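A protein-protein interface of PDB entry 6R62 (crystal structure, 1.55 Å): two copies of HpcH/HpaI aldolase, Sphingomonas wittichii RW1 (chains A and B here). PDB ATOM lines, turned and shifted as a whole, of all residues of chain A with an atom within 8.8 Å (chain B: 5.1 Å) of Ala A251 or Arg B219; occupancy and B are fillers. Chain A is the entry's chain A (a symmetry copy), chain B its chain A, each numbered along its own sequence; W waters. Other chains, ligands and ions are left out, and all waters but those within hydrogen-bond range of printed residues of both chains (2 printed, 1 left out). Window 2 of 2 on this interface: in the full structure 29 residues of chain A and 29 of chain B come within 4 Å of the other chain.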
ATOM      1  N   GLN A 244     -26.210 -34.228 -16.204  1.00  0.00           N
ATOM      2  CA  GLN A 244     -26.217 -33.687 -17.560  1.00  0.00           C
ATOM      3  C   GLN A 244     -25.386 -32.417 -17.657  1.00  0.00           C
ATOM      4  O   GLN A 244     -24.678 -32.206 -18.650  1.00  0.00           O
ATOM      5  CB  GLN A 244     -27.653 -33.431 -18.024  1.00  0.00           C
ATOM      6  CG  GLN A 244     -27.743 -33.063 -19.493  1.00  0.00           C
ATOM      7  CD  GLN A 244     -27.218 -34.165 -20.394  1.00  0.00           C
ATOM      8  OE1 GLN A 244     -27.594 -35.326 -20.253  1.00  0.00           O
ATOM      9  NE2 GLN A 244     -26.336 -33.807 -21.315  1.00  0.00           N
ATOM     10  N   VAL A 245     -25.460 -31.546 -16.645  1.00  0.00           N
ATOM     11  CA  VAL A 245     -24.634 -30.342 -16.649  1.00  0.00           C
ATOM     12  C   VAL A 245     -23.161 -30.718 -16.709  1.00  0.00           C
ATOM     13  O   VAL A 245     -22.381 -30.120 -17.452  1.00  0.00           O
ATOM     14  CB  VAL A 245     -24.950 -29.469 -15.419  1.00  0.00           C
ATOM     15  CG1 VAL A 245     -23.899 -28.403 -15.217  1.00  0.00           C
ATOM     16  CG2 VAL A 245     -26.307 -28.812 -15.563  1.00  0.00           C
ATOM     17  N   ILE A 246     -22.763 -31.732 -15.935  1.00  0.00           N
ATOM     18  CA  ILE A 246     -21.366 -32.157 -15.926  1.00  0.00           C
ATOM     19  C   ILE A 246     -20.976 -32.705 -17.288  1.00  0.00           C
ATOM     20  O   ILE A 246     -19.913 -32.376 -17.830  1.00  0.00           O
ATOM     21  CB  ILE A 246     -21.132 -33.190 -14.811  1.00  0.00           C
ATOM     22  CG1 ILE A 246     -21.272 -32.526 -13.439  1.00  0.00           C
ATOM     23  CG2 ILE A 246     -19.773 -33.850 -14.961  1.00  0.00           C
ATOM     24  CD1 ILE A 246     -21.404 -33.515 -12.307  1.00  0.00           C
ATOM     25  N   ALA A 247     -21.835 -33.548 -17.867  1.00  0.00           N
ATOM     26  CA  ALA A 247     -21.532 -34.117 -19.178  1.00  0.00           C
ATOM     27  C   ALA A 247     -21.363 -33.023 -20.222  1.00  0.00           C
ATOM     28  O   ALA A 247     -20.422 -33.061 -21.032  1.00  0.00           O
ATOM     29  CB  ALA A 247     -22.637 -35.081 -19.594  1.00  0.00           C
ATOM     30  N   ASP A 248     -22.256 -32.035 -20.211  1.00  0.00           N
ATOM     31  CA  ASP A 248     -22.159 -30.916 -21.138  1.00  0.00           C
ATOM     32  C   ASP A 248     -20.904 -30.086 -20.891  1.00  0.00           C
ATOM     33  O   ASP A 248     -20.282 -29.602 -21.836  1.00  0.00           O
ATOM     34  CB  ASP A 248     -23.392 -30.028 -21.011  1.00  0.00           C
ATOM     35  CG  ASP A 248     -24.661 -30.726 -21.462  1.00  0.00           C
ATOM     36  OD1 ASP A 248     -24.554 -31.773 -22.138  1.00  0.00           O
ATOM     37  OD2 ASP A 248     -25.763 -30.224 -21.156  1.00  0.00           O
ATOM     38  N   ALA A 249     -20.548 -29.877 -19.623  1.00  0.00           N
ATOM     39  CA  ALA A 249     -19.415 -29.026 -19.283  1.00  0.00           C
ATOM     40  C   ALA A 249     -18.098 -29.688 -19.654  1.00  0.00           C
ATOM     41  O   ALA A 249     -17.148 -29.006 -20.044  1.00  0.00           O
ATOM     42  CB  ALA A 249     -19.444 -28.699 -17.790  1.00  0.00           C
ATOM     43  N   ARG A 250     -18.021 -31.011 -19.515  1.00  0.00           N
ATOM     44  CA  ARG A 250     -16.791 -31.757 -19.735  1.00  0.00           C
ATOM     45  C   ARG A 250     -16.660 -32.293 -21.154  1.00  0.00           C
ATOM     46  O   ARG A 250     -15.624 -32.870 -21.486  1.00  0.00           O
ATOM     47  CB  ARG A 250     -16.699 -32.922 -18.749  1.00  0.00           C
ATOM     48  CG  ARG A 250     -16.581 -32.509 -17.280  1.00  0.00           C
ATOM     49  CD  ARG A 250     -16.120 -33.687 -16.448  1.00  0.00           C
ATOM     50  NE  ARG A 250     -15.900 -33.375 -15.035  1.00  0.00           N
ATOM     51  CZ  ARG A 250     -14.817 -32.765 -14.557  1.00  0.00           C
ATOM     52  NH1 ARG A 250     -13.856 -32.348 -15.367  1.00  0.00           N
ATOM     53  NH2 ARG A 250     -14.707 -32.570 -13.251  1.00  0.00           N
ATOM     54  N   ALA A 251     -17.679 -32.131 -21.990  1.00  0.00           N
ATOM     55  CA  ALA A 251     -17.580 -32.574 -23.373  1.00  0.00           C
ATOM     56  C   ALA A 251     -16.525 -31.770 -24.123  1.00  0.00           C
ATOM     57  O   ALA A 251     -16.267 -30.600 -23.827  1.00  0.00           O
ATOM     58  CB  ALA A 251     -18.931 -32.439 -24.070  1.00  0.00           C
ATOM     59  N   LEU A 252     -15.904 -32.408 -25.103  1.00  0.00           N
ATOM     60  CA  LEU A 252     -14.974 -31.690 -25.961  1.00  0.00           C
ATOM     61  C   LEU A 252     -15.724 -30.609 -26.727  1.00  0.00           C
ATOM     62  O   LEU A 252     -15.183 -29.531 -26.992  1.00  0.00           O
ATOM     63  CB  LEU A 252     -14.283 -32.644 -26.930  1.00  0.00           C
ATOM     64  CG  LEU A 252     -13.310 -33.645 -26.309  1.00  0.00           C
ATOM     65  CD1 LEU A 252     -12.887 -34.661 -27.361  1.00  0.00           C
ATOM     66  CD2 LEU A 252     -12.095 -32.927 -25.732  1.00  0.00           C
ATOM     67  OXT LEU A 252     -16.885 -30.804 -27.095  1.00  0.00           O
ATOM     68  N   GLY B 215     -24.322 -25.940 -18.274  1.00  0.00           N
ATOM     69  CA  GLY B 215     -23.202 -26.769 -18.682  1.00  0.00           C
ATOM     70  C   GLY B 215     -22.549 -26.304 -19.971  1.00  0.00           C
ATOM     71  O   GLY B 215     -21.328 -26.412 -20.122  1.00  0.00           O
ATOM     72  N   GLY B 216     -23.338 -25.773 -20.906  1.00  0.00           N
ATOM     73  CA  GLY B 216     -22.761 -25.260 -22.142  1.00  0.00           C
ATOM     74  C   GLY B 216     -21.884 -24.036 -21.946  1.00  0.00           C
ATOM     75  O   GLY B 216     -20.838 -23.901 -22.590  1.00  0.00           O
ATOM     76  N   PHE B 217     -22.303 -23.108 -21.082  1.00  0.00           N
ATOM     77  CA  PHE B 217     -21.461 -21.949 -20.811  1.00  0.00           C
ATOM     78  C   PHE B 217     -20.198 -22.374 -20.082  1.00  0.00           C
ATOM     79  O   PHE B 217     -19.100 -21.905 -20.400  1.00  0.00           O
ATOM     80  CB  PHE B 217     -22.252 -20.921 -20.004  1.00  0.00           C
ATOM     81  CG  PHE B 217     -21.534 -19.612 -19.780  1.00  0.00           C
ATOM     82  CD1 PHE B 217     -21.642 -18.574 -20.692  1.00  0.00           C
ATOM     83  CD2 PHE B 217     -20.802 -19.407 -18.622  1.00  0.00           C
ATOM     84  CE1 PHE B 217     -20.997 -17.360 -20.464  1.00  0.00           C
ATOM     85  CE2 PHE B 217     -20.155 -18.203 -18.391  1.00  0.00           C
ATOM     86  CZ  PHE B 217     -20.260 -17.181 -19.310  1.00  0.00           C
ATOM     87  N   ALA B 218     -20.336 -23.303 -19.133  1.00  0.00           N
ATOM     88  CA  ALA B 218     -19.173 -23.839 -18.433  1.00  0.00           C
ATOM     89  C   ALA B 218     -18.177 -24.468 -19.399  1.00  0.00           C
ATOM     90  O   ALA B 218     -16.970 -24.304 -19.230  1.00  0.00           O
ATOM     91  CB  ALA B 218     -19.624 -24.863 -17.396  1.00  0.00           C
ATOM     92  N   ARG B 219     -18.659 -25.217 -20.401  1.00  0.00           N
ATOM     93  CA  ARG B 219     -17.739 -25.790 -21.382  1.00  0.00           C
ATOM     94  C   ARG B 219     -16.948 -24.699 -22.087  1.00  0.00           C
ATOM     95  O   ARG B 219     -15.737 -24.833 -22.301  1.00  0.00           O
ATOM     96  CB  ARG B 219     -18.490 -26.644 -22.418  1.00  0.00           C
ATOM     97  CG  ARG B 219     -17.567 -27.215 -23.522  1.00  0.00           C
ATOM     98  CD  ARG B 219     -18.322 -28.051 -24.554  1.00  0.00           C
ATOM     99  NE  ARG B 219     -19.394 -27.284 -25.175  1.00  0.00           N
ATOM    100  CZ  ARG B 219     -19.208 -26.284 -26.031  1.00  0.00           C
ATOM    101  NH1 ARG B 219     -17.981 -25.916 -26.388  1.00  0.00           N
ATOM    102  NH2 ARG B 219     -20.257 -25.646 -26.529  1.00  0.00           N
ATOM    103  N   VAL B 220     -17.619 -23.617 -22.484  1.00  0.00           N
ATOM    104  CA  VAL B 220     -16.917 -22.527 -23.152  1.00  0.00           C
ATOM    105  C   VAL B 220     -15.898 -21.892 -22.212  1.00  0.00           C
ATOM    106  O   VAL B 220     -14.777 -21.581 -22.621  1.00  0.00           O
ATOM    107  CB  VAL B 220     -17.923 -21.492 -23.683  1.00  0.00           C
ATOM    108  CG1 VAL B 220     -17.197 -20.292 -24.269  1.00  0.00           C
ATOM    109  CG2 VAL B 220     -18.820 -22.129 -24.745  1.00  0.00           C
ATOM    110  N   LYS B 221     -16.262 -21.693 -20.941  1.00  0.00           N
ATOM    111  CA  LYS B 221     -15.307 -21.097 -20.005  1.00  0.00           C
ATOM    112  C   LYS B 221     -14.081 -21.983 -19.823  1.00  0.00           C
ATOM    113  O   LYS B 221     -12.956 -21.484 -19.721  1.00  0.00           O
ATOM    114  CB  LYS B 221     -15.956 -20.834 -18.653  1.00  0.00           C
ATOM    115  CG  LYS B 221     -17.153 -19.889 -18.684  1.00  0.00           C
ATOM    116  CD  LYS B 221     -16.853 -18.564 -19.370  1.00  0.00           C
ATOM    117  CE  LYS B 221     -17.352 -18.529 -20.806  1.00  0.00           C
ATOM    118  NZ  LYS B 221     -17.234 -17.184 -21.442  1.00  0.00           N
ATOM    119  N   LEU B 222     -14.271 -23.301 -19.782  1.00  0.00           N
ATOM    120  CA  LEU B 222     -13.114 -24.185 -19.693  1.00  0.00           C
ATOM    121  C   LEU B 222     -12.242 -24.065 -20.935  1.00  0.00           C
ATOM    122  O   LEU B 222     -11.010 -24.010 -20.841  1.00  0.00           O
ATOM    123  CB  LEU B 222     -13.570 -25.629 -19.474  1.00  0.00           C
ATOM    124  CG  LEU B 222     -14.236 -25.896 -18.118  1.00  0.00           C
ATOM    125  CD1 LEU B 222     -14.961 -27.242 -18.081  1.00  0.00           C
ATOM    126  CD2 LEU B 222     -13.216 -25.827 -17.003  1.00  0.00           C
ATOM    127  N   ALA B 223     -12.865 -23.987 -22.114  1.00  0.00           N
ATOM    128  CA  ALA B 223     -12.102 -23.808 -23.341  1.00  0.00           C
ATOM    129  C   ALA B 223     -11.330 -22.492 -23.342  1.00  0.00           C
ATOM    130  O   ALA B 223     -10.235 -22.417 -23.913  1.00  0.00           O
ATOM    131  CB  ALA B 223     -13.044 -23.874 -24.544  1.00  0.00           C
HETATM  132  O   HOH W   1     -15.183 -27.176 -25.797  1.00  0.00           O
HETATM  133  O   HOH W   2     -21.521 -29.100 -24.213  1.00  0.00           O
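OD1 of Asp A248 lies within hydrogen-bond range of NE2 of Gln A244 (2.8 Å).
Val A245 touches Gly B215. O of Asp A248 touches O of Gly B215 (3.8 Å). CB of Arg B219 touches O of Asp A248 (3.5 Å). Ala A249 touches Gly B215. CB of Ala A249 touches CB of Ala B218 (3.9 Å). Ala A249 touches Arg B219. CD1 of Leu B222 touches O of Ala A249, 3.4 Å away. Ala A251 touches Arg B219.
Of chain B, only Arg B219 comes within 4 Å of Ala A251. Ala B218 touches just one residue of chain A: Ala A249. Printed residues of chain B within 4 Å of Val A245: Gly B215. Of the printed residues of chain A, Gly B215 touches Val A245 (3.7 Å), Asp A248 (3.8 Å) and Ala A249 (3.3 Å). Of the printed residues of chain B, Ala A249 touches Gly B215, Ala B218, Arg B219 and Leu B222. Ala B223 touches none of the printed residues of chain A. The nearest printed residue of chain A that does not touch Arg B219 is Leu A252 (4.01 Å).
Of the 9 printed residues of chain A, 4 touch a printed residue of chain B. Of the 9 printed residues of chain B, 4 touch a printed residue of chain A.
No position is printed for both chains. Of the 8 pairs that touch across the chains among the printed residues, none has its exchanged pair printed and touching as well.
Water W1 lies within hydrogen-bond range of O of Leu A252 (2.6 Å) and NH1 of Arg B219 (3.1 Å). Water W2 lies within hydrogen-bond range of the backbone carbonyl oxygen of Asp A248 and the guanidinium group of Arg B219.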
